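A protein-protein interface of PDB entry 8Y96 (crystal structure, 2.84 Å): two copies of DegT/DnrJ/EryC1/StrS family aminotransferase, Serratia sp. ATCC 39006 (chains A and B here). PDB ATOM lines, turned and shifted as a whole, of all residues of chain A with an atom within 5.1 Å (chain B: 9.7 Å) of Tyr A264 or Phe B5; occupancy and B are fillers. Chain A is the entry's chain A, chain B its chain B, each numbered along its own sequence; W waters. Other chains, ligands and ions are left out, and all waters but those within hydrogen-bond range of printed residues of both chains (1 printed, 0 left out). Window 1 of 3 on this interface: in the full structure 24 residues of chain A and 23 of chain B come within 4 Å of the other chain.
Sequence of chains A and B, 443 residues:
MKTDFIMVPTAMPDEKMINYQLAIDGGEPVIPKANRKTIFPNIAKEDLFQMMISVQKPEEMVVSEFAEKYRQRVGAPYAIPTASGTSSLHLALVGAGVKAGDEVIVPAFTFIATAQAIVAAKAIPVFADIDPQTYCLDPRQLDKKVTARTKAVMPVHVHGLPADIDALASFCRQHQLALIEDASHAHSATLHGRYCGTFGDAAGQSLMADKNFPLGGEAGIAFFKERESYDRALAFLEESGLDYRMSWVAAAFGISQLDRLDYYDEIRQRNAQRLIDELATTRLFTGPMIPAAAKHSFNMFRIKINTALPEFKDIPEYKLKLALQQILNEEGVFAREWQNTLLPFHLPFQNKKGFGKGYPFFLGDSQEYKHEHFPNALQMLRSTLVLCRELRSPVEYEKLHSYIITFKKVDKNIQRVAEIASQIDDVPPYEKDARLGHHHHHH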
ATOM      1  N   ASN A  42      16.779   2.712  24.993  1.00  0.00           N
ATOM      2  CA  ASN A  42      15.368   2.882  24.694  1.00  0.00           C
ATOM      3  C   ASN A  42      14.558   2.618  25.959  1.00  0.00           C
ATOM      4  O   ASN A  42      13.989   1.546  26.121  1.00  0.00           O
ATOM      5  CB  ASN A  42      14.930   1.981  23.543  1.00  0.00           C
ATOM      6  CG  ASN A  42      15.802   2.154  22.321  1.00  0.00           C
ATOM      7  OD1 ASN A  42      15.712   3.177  21.636  1.00  0.00           O
ATOM      8  ND2 ASN A  42      16.647   1.174  22.028  1.00  0.00           N
ATOM      9  N   ALA A  44      11.602   2.444  27.981  1.00  0.00           N
ATOM     10  CA  ALA A  44      10.169   2.411  27.758  1.00  0.00           C
ATOM     11  C   ALA A  44       9.453   2.184  29.085  1.00  0.00           C
ATOM     12  O   ALA A  44      10.099   1.970  30.109  1.00  0.00           O
ATOM     13  CB  ALA A  44       9.842   1.331  26.751  1.00  0.00           C
ATOM     14  N   GLU A  46       7.917  -0.270  30.179  1.00  0.00           N
ATOM     15  CA  GLU A  46       8.163  -1.596  30.725  1.00  0.00           C
ATOM     16  C   GLU A  46       9.327  -1.562  31.715  1.00  0.00           C
ATOM     17  O   GLU A  46       9.348  -2.331  32.667  1.00  0.00           O
ATOM     18  CB  GLU A  46       8.443  -2.606  29.609  1.00  0.00           C
ATOM     19  CG  GLU A  46       7.227  -2.936  28.744  1.00  0.00           C
ATOM     20  CD  GLU A  46       6.817  -1.901  27.707  1.00  0.00           C
ATOM     21  OE1 GLU A  46       7.578  -0.942  27.475  1.00  0.00           O
ATOM     22  OE2 GLU A  46       5.720  -2.051  27.130  1.00  0.00           O
ATOM     23  N   GLN A 257      14.893  -5.026  29.643  1.00  0.00           N
ATOM     24  CA  GLN A 257      15.535  -4.725  28.375  1.00  0.00           C
ATOM     25  C   GLN A 257      15.705  -5.999  27.553  1.00  0.00           C
ATOM     26  O   GLN A 257      15.725  -5.937  26.323  1.00  0.00           O
ATOM     27  CB  GLN A 257      16.901  -4.069  28.574  1.00  0.00           C
ATOM     28  CG  GLN A 257      16.845  -2.588  28.932  1.00  0.00           C
ATOM     29  CD  GLN A 257      16.569  -1.694  27.743  1.00  0.00           C
ATOM     30  OE1 GLN A 257      17.128  -1.880  26.654  1.00  0.00           O
ATOM     31  NE2 GLN A 257      15.697  -0.713  27.940  1.00  0.00           N
ATOM     32  N   ARG A 260      12.956  -7.140  25.117  1.00  0.00           N
ATOM     33  CA  ARG A 260      12.776  -6.325  23.922  1.00  0.00           C
ATOM     34  C   ARG A 260      14.047  -6.287  23.070  1.00  0.00           C
ATOM     35  O   ARG A 260      14.090  -5.567  22.078  1.00  0.00           O
ATOM     36  CB  ARG A 260      12.353  -4.899  24.300  1.00  0.00           C
ATOM     37  CG  ARG A 260      11.237  -4.814  25.334  1.00  0.00           C
ATOM     38  CD  ARG A 260      10.492  -3.485  25.314  1.00  0.00           C
ATOM     39  NE  ARG A 260      11.352  -2.302  25.456  1.00  0.00           N
ATOM     40  CZ  ARG A 260      11.969  -1.908  26.570  1.00  0.00           C
ATOM     41  NH1 ARG A 260      11.797  -2.568  27.704  1.00  0.00           N
ATOM     42  NH2 ARG A 260      12.757  -0.846  26.545  1.00  0.00           N
ATOM     43  N   LEU A 261      15.069  -7.074  23.423  1.00  0.00           N
ATOM     44  CA  LEU A 261      16.374  -6.941  22.791  1.00  0.00           C
ATOM     45  C   LEU A 261      16.335  -7.420  21.336  1.00  0.00           C
ATOM     46  O   LEU A 261      17.075  -6.909  20.499  1.00  0.00           O
ATOM     47  CB  LEU A 261      17.434  -7.687  23.600  1.00  0.00           C
ATOM     48  CG  LEU A 261      18.803  -7.855  22.930  1.00  0.00           C
ATOM     49  CD1 LEU A 261      19.458  -6.521  22.617  1.00  0.00           C
ATOM     50  CD2 LEU A 261      19.716  -8.696  23.798  1.00  0.00           C
ATOM     51  N   ASP A 262      15.495  -8.412  21.027  1.00  0.00           N
ATOM     52  CA  ASP A 262      15.472  -8.969  19.680  1.00  0.00           C
ATOM     53  C   ASP A 262      14.835  -7.974  18.714  1.00  0.00           C
ATOM     54  O   ASP A 262      15.236  -7.896  17.554  1.00  0.00           O
ATOM     55  CB  ASP A 262      14.817 -10.341  19.641  1.00  0.00           C
ATOM     56  CG  ASP A 262      15.603 -11.443  20.337  1.00  0.00           C
ATOM     57  OD1 ASP A 262      16.847 -11.474  20.177  1.00  0.00           O
ATOM     58  OD2 ASP A 262      14.964 -12.265  21.020  1.00  0.00           O
ATOM     59  N   TYR A 263      13.848  -7.218  19.210  1.00  0.00           N
ATOM     60  CA  TYR A 263      13.206  -6.172  18.434  1.00  0.00           C
ATOM     61  C   TYR A 263      14.234  -5.120  18.025  1.00  0.00           C
ATOM     62  O   TYR A 263      14.398  -4.839  16.842  1.00  0.00           O
ATOM     63  CB  TYR A 263      12.066  -5.552  19.242  1.00  0.00           C
ATOM     64  CG  TYR A 263      11.447  -4.330  18.580  1.00  0.00           C
ATOM     65  CD1 TYR A 263      10.587  -4.464  17.498  1.00  0.00           C
ATOM     66  CD2 TYR A 263      11.718  -3.048  19.040  1.00  0.00           C
ATOM     67  CE1 TYR A 263      10.012  -3.361  16.892  1.00  0.00           C
ATOM     68  CE2 TYR A 263      11.148  -1.935  18.443  1.00  0.00           C
ATOM     69  CZ  TYR A 263      10.292  -2.093  17.366  1.00  0.00           C
ATOM     70  OH  TYR A 263       9.725  -1.018  16.757  1.00  0.00           O
ATOM     71  N   TYR A 264      14.929  -4.553  19.014  1.00  0.00           N
ATOM     72  CA  TYR A 264      15.901  -3.499  18.768  1.00  0.00           C
ATOM     73  C   TYR A 264      17.047  -4.024  17.904  1.00  0.00           C
ATOM     74  O   TYR A 264      17.564  -3.290  17.069  1.00  0.00           O
ATOM     75  CB  TYR A 264      16.405  -2.940  20.101  1.00  0.00           C
ATOM     76  CG  TYR A 264      15.342  -2.258  20.954  1.00  0.00           C
ATOM     77  CD1 TYR A 264      14.471  -1.316  20.414  1.00  0.00           C
ATOM     78  CD2 TYR A 264      15.201  -2.569  22.302  1.00  0.00           C
ATOM     79  CE1 TYR A 264      13.509  -0.692  21.193  1.00  0.00           C
ATOM     80  CE2 TYR A 264      14.238  -1.958  23.090  1.00  0.00           C
ATOM     81  CZ  TYR A 264      13.392  -1.015  22.535  1.00  0.00           C
ATOM     82  OH  TYR A 264      12.443  -0.421  23.313  1.00  0.00           O
ATOM     83  N   ASP A 265      17.434  -5.291  18.107  1.00  0.00           N
ATOM     84  CA  ASP A 265      18.499  -5.916  17.333  1.00  0.00           C
ATOM     85  C   ASP A 265      18.133  -5.940  15.849  1.00  0.00           C
ATOM     86  O   ASP A 265      18.971  -5.644  14.998  1.00  0.00           O
ATOM     87  CB  ASP A 265      18.803  -7.321  17.834  1.00  0.00           C
ATOM     88  CG  ASP A 265      19.792  -7.434  18.987  1.00  0.00           C
ATOM     89  OD1 ASP A 265      20.457  -6.425  19.301  1.00  0.00           O
ATOM     90  OD2 ASP A 265      19.896  -8.541  19.561  1.00  0.00           O
ATOM     91  N   GLU A 266      16.876  -6.300  15.558  1.00  0.00           N
ATOM     92  CA  GLU A 266      16.397  -6.457  14.192  1.00  0.00           C
ATOM     93  C   GLU A 266      16.560  -5.147  13.421  1.00  0.00           C
ATOM     94  O   GLU A 266      17.037  -5.157  12.289  1.00  0.00           O
ATOM     95  CB  GLU A 266      14.955  -6.968  14.231  1.00  0.00           C
ATOM     96  CG  GLU A 266      14.323  -7.199  12.860  1.00  0.00           C
ATOM     97  CD  GLU A 266      14.989  -8.225  11.958  1.00  0.00           C
ATOM     98  OE1 GLU A 266      15.914  -8.935  12.407  1.00  0.00           O
ATOM     99  OE2 GLU A 266      14.574  -8.309  10.782  1.00  0.00           O
ATOM    100  N   ILE A 267      16.174  -4.025  14.041  1.00  0.00           N
ATOM    101  CA  ILE A 267      16.301  -2.718  13.416  1.00  0.00           C
ATOM    102  C   ILE A 267      17.786  -2.388  13.250  1.00  0.00           C
ATOM    103  O   ILE A 267      18.220  -1.977  12.176  1.00  0.00           O
ATOM    104  CB  ILE A 267      15.541  -1.643  14.221  1.00  0.00           C
ATOM    105  CG1 ILE A 267      14.050  -1.964  14.314  1.00  0.00           C
ATOM    106  CG2 ILE A 267      15.771  -0.248  13.639  1.00  0.00           C
ATOM    107  CD1 ILE A 267      13.273  -1.067  15.264  1.00  0.00           C
ATOM    108  N   ARG A 268      18.569  -2.581  14.313  1.00  0.00           N
ATOM    109  CA  ARG A 268      20.011  -2.402  14.231  1.00  0.00           C
ATOM    110  C   ARG A 268      20.549  -3.080  12.969  1.00  0.00           C
ATOM    111  O   ARG A 268      21.287  -2.454  12.208  1.00  0.00           O
ATOM    112  CB  ARG A 268      20.713  -2.899  15.503  1.00  0.00           C
ATOM    113  CG  ARG A 268      21.272  -1.794  16.392  1.00  0.00           C
ATOM    114  CD  ARG A 268      21.765  -2.296  17.747  1.00  0.00           C
ATOM    115  NE  ARG A 268      20.903  -1.897  18.866  1.00  0.00           N
ATOM    116  CZ  ARG A 268      20.243  -2.677  19.727  1.00  0.00           C
ATOM    117  NH1 ARG A 268      20.211  -3.992  19.590  1.00  0.00           N
ATOM    118  NH2 ARG A 268      19.582  -2.119  20.732  1.00  0.00           N
ATOM    119  N   PRO A 394      18.498   2.305  17.632  1.00  0.00           N
ATOM    120  CA  PRO A 394      17.752   1.714  16.520  1.00  0.00           C
ATOM    121  C   PRO A 394      16.907   2.757  15.793  1.00  0.00           C
ATOM    122  O   PRO A 394      15.690   2.803  15.962  1.00  0.00           O
ATOM    123  CB  PRO A 394      16.907   0.661  17.241  1.00  0.00           C
ATOM    124  CG  PRO A 394      16.590   1.321  18.564  1.00  0.00           C
ATOM    125  CD  PRO A 394      17.889   2.016  18.938  1.00  0.00           C
ATOM    126  N   MET B   1       4.851 -10.079  33.157  1.00  0.00           N
ATOM    127  CA  MET B   1       4.518  -8.679  32.786  1.00  0.00           C
ATOM    128  C   MET B   1       3.719  -8.679  31.486  1.00  0.00           C
ATOM    129  O   MET B   1       4.264  -8.980  30.426  1.00  0.00           O
ATOM    130  CB  MET B   1       5.788  -7.839  32.607  1.00  0.00           C
ATOM    131  CG  MET B   1       5.527  -6.412  32.163  1.00  0.00           C
ATOM    132  SD  MET B   1       7.016  -5.397  32.160  1.00  0.00           S
ATOM    133  CE  MET B   1       7.879  -6.105  30.749  1.00  0.00           C
ATOM    134  N   LYS B   2       2.429  -8.340  31.587  1.00  0.00           N
ATOM    135  CA  LYS B   2       1.585  -8.204  30.414  1.00  0.00           C
ATOM    136  C   LYS B   2       1.897  -6.858  29.765  1.00  0.00           C
ATOM    137  O   LYS B   2       1.685  -5.815  30.384  1.00  0.00           O
ATOM    138  CB  LYS B   2       0.096  -8.308  30.769  1.00  0.00           C
ATOM    139  CG  LYS B   2      -0.798  -8.811  29.634  1.00  0.00           C
ATOM    140  CD  LYS B   2      -2.041  -7.972  29.356  1.00  0.00           C
ATOM    141  CE  LYS B   2      -3.005  -7.852  30.495  1.00  0.00           C
ATOM    142  NZ  LYS B   2      -3.783  -9.077  30.691  1.00  0.00           N
ATOM    143  N   THR B   3       2.411  -6.896  28.528  1.00  0.00           N
ATOM    144  CA  THR B   3       2.802  -5.697  27.803  1.00  0.00           C
ATOM    145  C   THR B   3       2.208  -5.736  26.395  1.00  0.00           C
ATOM    146  O   THR B   3       1.971  -6.810  25.846  1.00  0.00           O
ATOM    147  CB  THR B   3       4.326  -5.575  27.766  1.00  0.00           C
ATOM    148  OG1 THR B   3       4.598  -4.551  26.814  1.00  0.00           O
ATOM    149  CG2 THR B   3       5.029  -6.850  27.336  1.00  0.00           C
ATOM    150  N   ASP B   4       1.993  -4.546  25.817  1.00  0.00           N
ATOM    151  CA  ASP B   4       1.478  -4.417  24.463  1.00  0.00           C
ATOM    152  C   ASP B   4       2.630  -4.289  23.466  1.00  0.00           C
ATOM    153  O   ASP B   4       2.396  -4.255  22.260  1.00  0.00           O
ATOM    154  CB  ASP B   4       0.495  -3.262  24.347  1.00  0.00           C
ATOM    155  CG  ASP B   4       1.056  -1.874  24.620  1.00  0.00           C
ATOM    156  OD1 ASP B   4       2.210  -1.780  25.093  1.00  0.00           O
ATOM    157  OD2 ASP B   4       0.337  -0.893  24.351  1.00  0.00           O
ATOM    158  N   PHE B   5       3.872  -4.223  23.967  1.00  0.00           N
ATOM    159  CA  PHE B   5       5.037  -3.989  23.128  1.00  0.00           C
ATOM    160  C   PHE B   5       5.011  -4.929  21.924  1.00  0.00           C
ATOM    161  O   PHE B   5       4.952  -6.147  22.084  1.00  0.00           O
ATOM    162  CB  PHE B   5       6.341  -4.173  23.909  1.00  0.00           C
ATOM    163  CG  PHE B   5       7.562  -3.644  23.169  1.00  0.00           C
ATOM    164  CD1 PHE B   5       7.855  -2.285  23.168  1.00  0.00           C
ATOM    165  CD2 PHE B   5       8.404  -4.498  22.466  1.00  0.00           C
ATOM    166  CE1 PHE B   5       8.959  -1.795  22.489  1.00  0.00           C
ATOM    167  CE2 PHE B   5       9.509  -4.001  21.787  1.00  0.00           C
ATOM    168  CZ  PHE B   5       9.783  -2.652  21.801  1.00  0.00           C
ATOM    169  N   ILE B   6       5.049  -4.336  20.723  1.00  0.00           N
ATOM    170  CA  ILE B   6       5.140  -5.081  19.478  1.00  0.00           C
ATOM    171  C   ILE B   6       6.595  -5.508  19.286  1.00  0.00           C
ATOM    172  O   ILE B   6       7.490  -4.669  19.328  1.00  0.00           O
ATOM    173  CB  ILE B   6       4.603  -4.234  18.307  1.00  0.00           C
ATOM    174  CG1 ILE B   6       3.113  -3.919  18.498  1.00  0.00           C
ATOM    175  CG2 ILE B   6       4.867  -4.907  16.960  1.00  0.00           C
ATOM    176  CD1 ILE B   6       2.576  -2.820  17.596  1.00  0.00           C
ATOM    177  N   MET B   7       6.812  -6.816  19.079  1.00  0.00           N
ATOM    178  CA  MET B   7       8.142  -7.411  19.118  1.00  0.00           C
ATOM    179  C   MET B   7       8.754  -7.531  17.723  1.00  0.00           C
ATOM    180  O   MET B   7       9.964  -7.703  17.604  1.00  0.00           O
ATOM    181  CB  MET B   7       8.102  -8.812  19.740  1.00  0.00           C
ATOM    182  CG  MET B   7       7.978  -8.832  21.255  1.00  0.00           C
ATOM    183  SD  MET B   7       9.316  -7.983  22.116  1.00  0.00           S
ATOM    184  CE  MET B   7      10.798  -8.621  21.318  1.00  0.00           C
ATOM    185  N   VAL B   8       7.925  -7.458  16.675  1.00  0.00           N
ATOM    186  CA  VAL B   8       8.393  -7.662  15.312  1.00  0.00           C
ATOM    187  C   VAL B   8       8.289  -6.329  14.576  1.00  0.00           C
ATOM    188  O   VAL B   8       7.190  -5.804  14.408  1.00  0.00           O
ATOM    189  CB  VAL B   8       7.599  -8.761  14.572  1.00  0.00           C
ATOM    190  CG1 VAL B   8       8.231  -9.107  13.228  1.00  0.00           C
ATOM    191  CG2 VAL B   8       7.424 -10.022  15.413  1.00  0.00           C
ATOM    192  N   PRO B   9       9.413  -5.740  14.107  1.00  0.00           N
ATOM    193  CA  PRO B   9       9.358  -4.477  13.372  1.00  0.00           C
ATOM    194  C   PRO B   9       8.739  -4.705  11.998  1.00  0.00           C
ATOM    195  O   PRO B   9       8.846  -5.797  11.446  1.00  0.00           O
ATOM    196  CB  PRO B   9      10.822  -4.019  13.295  1.00  0.00           C
ATOM    197  CG  PRO B   9      11.620  -5.297  13.408  1.00  0.00           C
ATOM    198  CD  PRO B   9      10.782  -6.265  14.232  1.00  0.00           C
ATOM    199  N   ALA B  34       1.895 -10.564  11.506  1.00  0.00           N
ATOM    200  CA  ALA B  34       2.646 -10.074  12.652  1.00  0.00           C
ATOM    201  C   ALA B  34       2.642  -8.544  12.714  1.00  0.00           C
ATOM    202  O   ALA B  34       2.616  -7.976  13.801  1.00  0.00           O
ATOM    203  CB  ALA B  34       4.059 -10.618  12.614  1.00  0.00           C
ATOM    204  N   LYS B  37      -0.782  -5.133  13.948  1.00  0.00           N
ATOM    205  CA  LYS B  37      -1.213  -4.419  15.144  1.00  0.00           C
ATOM    206  C   LYS B  37      -0.533  -3.050  15.225  1.00  0.00           C
ATOM    207  O   LYS B  37       0.647  -2.919  14.898  1.00  0.00           O
ATOM    208  CB  LYS B  37      -0.912  -5.246  16.403  1.00  0.00           C
ATOM    209  CG  LYS B  37      -2.068  -5.359  17.396  1.00  0.00           C
ATOM    210  N   THR B  38      -1.298  -2.036  15.655  1.00  0.00           N
ATOM    211  CA  THR B  38      -0.762  -0.724  16.003  1.00  0.00           C
ATOM    212  C   THR B  38      -0.944  -0.511  17.502  1.00  0.00           C
ATOM    213  O   THR B  38      -1.731  -1.211  18.137  1.00  0.00           O
ATOM    214  CB  THR B  38      -1.447   0.398  15.219  1.00  0.00           C
ATOM    215  OG1 THR B  38      -2.848   0.241  15.428  1.00  0.00           O
ATOM    216  CG2 THR B  38      -1.118   0.370  13.738  1.00  0.00           C
ATOM    217  N   ILE B  39      -0.220   0.476  18.043  1.00  0.00           N
ATOM    218  CA  ILE B  39      -0.275   0.814  19.460  1.00  0.00           C
ATOM    219  C   ILE B  39      -1.002   2.144  19.629  1.00  0.00           C
ATOM    220  O   ILE B  39      -0.633   3.140  19.005  1.00  0.00           O
ATOM    221  CB  ILE B  39       1.144   0.867  20.060  1.00  0.00           C
ATOM    222  CG1 ILE B  39       1.708  -0.537  20.279  1.00  0.00           C
ATOM    223  CG2 ILE B  39       1.188   1.696  21.346  1.00  0.00           C
ATOM    224  CD1 ILE B  39       0.804  -1.457  21.081  1.00  0.00           C
ATOM    225  N   PHE B  40      -2.017   2.155  20.500  1.00  0.00           N
ATOM    226  CA  PHE B  40      -2.645   3.414  20.860  1.00  0.00           C
ATOM    227  C   PHE B  40      -3.366   3.272  22.200  1.00  0.00           C
ATOM    228  O   PHE B  40      -4.165   2.356  22.380  1.00  0.00           O
ATOM    229  CB  PHE B  40      -3.595   3.913  19.767  1.00  0.00           C
ATOM    230  CG  PHE B  40      -3.820   5.412  19.872  1.00  0.00           C
ATOM    231  CD1 PHE B  40      -2.895   6.302  19.340  1.00  0.00           C
ATOM    232  CD2 PHE B  40      -4.917   5.924  20.554  1.00  0.00           C
ATOM    233  CE1 PHE B  40      -3.078   7.669  19.473  1.00  0.00           C
ATOM    234  CE2 PHE B  40      -5.096   7.292  20.679  1.00  0.00           C
ATOM    235  CZ  PHE B  40      -4.178   8.161  20.136  1.00  0.00           C
ATOM    236  N   PRO B  41      -3.160   4.198  23.169  1.00  0.00           N
ATOM    237  CA  PRO B  41      -2.341   5.396  22.976  1.00  0.00           C
ATOM    238  C   PRO B  41      -0.847   5.115  23.073  1.00  0.00           C
ATOM    239  O   PRO B  41      -0.437   3.992  23.358  1.00  0.00           O
ATOM    240  CB  PRO B  41      -2.816   6.339  24.098  1.00  0.00           C
ATOM    241  CG  PRO B  41      -3.999   5.639  24.739  1.00  0.00           C
ATOM    242  CD  PRO B  41      -3.754   4.160  24.511  1.00  0.00           C
ATOM    243  N   ILE B  43       1.762   5.146  25.162  1.00  0.00           N
ATOM    244  CA  ILE B  43       2.066   5.206  26.579  1.00  0.00           C
ATOM    245  C   ILE B  43       3.578   5.101  26.746  1.00  0.00           C
ATOM    246  O   ILE B  43       4.166   4.063  26.454  1.00  0.00           O
ATOM    247  CB  ILE B  43       1.298   4.120  27.356  1.00  0.00           C
ATOM    248  CG1 ILE B  43      -0.212   4.315  27.193  1.00  0.00           C
ATOM    249  CG2 ILE B  43       1.711   4.106  28.829  1.00  0.00           C
ATOM    250  CD1 ILE B  43      -1.071   3.336  27.969  1.00  0.00           C
HETATM  251  O   HOH W   1       4.558  -1.053  24.279  1.00  0.00           O
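Printed residues of chain B that touch a printed residue of chain A: Met B1, Thr B3, Phe B5, Ile B6, Met B7 and Pro B9. Of the 14 printed residues of chain A, 6 touch a printed residue of chain B. Hydrophobic or aromatic side chains of chain A that line the printed part of chain B: Tyr A263, Tyr A264 and Ile A267. Among the printed residues, no Asp or Glu carboxylate lies within 4 Å of a Lys or Arg side-chain nitrogen of the other chain.
Of chain A, only Glu A46, Arg A260, Tyr A263 and Tyr A264 come within 4 Å of Phe B5. No residue of chain B comes within 4 Å of Asp A265. Of the printed residues of chain B, Glu A46 touches Met B1, Thr B3 and Phe B5. Printed residues of chain A within 4 Å of Ile B6: Tyr A263. Of the printed residues of chain A, Met B1 touches Glu A46 (3.7 Å). Ala B34 touches none of the printed residues of chain A.
Among the printed residues, merely in contact across the chains: Tyr A263 with Met B7, Glu A266 with Pro B9, Tyr A263 with Phe B5, Tyr A263 with Ile B6, Arg A260 with Phe B5, Tyr A263 with Pro B9, Glu A46 with Met B1, Tyr A264 with Phe B5, Glu A46 with Phe B5, Ile A267 with Pro B9 and Arg A260 with Met B7.
The side-chain hydroxyl of Thr B3 is in hydrogen-bond range of the side-chain carboxylate of Glu A46, 2.8 Å away.
The side-chain hydroxyl (OH) of Tyr A264 is in hydrogen-bond range of the guanidinium group (NE) of Arg A260. The side-chain amide nitrogen of Gln A257 lies close to the guanidinium group of Arg A260, 3.3 Å away. The guanidinium group (NH2) of Arg A260 sits at hydrogen-bond distance from the backbone carbonyl oxygen (O) of Asn A42 (2.7 Å). The backbone NH (N) of Phe B5 is in hydrogen-bond range of the side-chain hydroxyl (OG1) of Thr B3, at 3.0 Å.
Water W1 lies within hydrogen-bond range of OD1 of Asp B4 (2.6 Å), OE2 of Glu A46 (3.2 Å) and N of Phe B5 (3.3 Å).
No position is printed for both chains. Of the 12 pairs that touch across the chains among the printed residues, none has its exchanged pair printed and touching as well.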
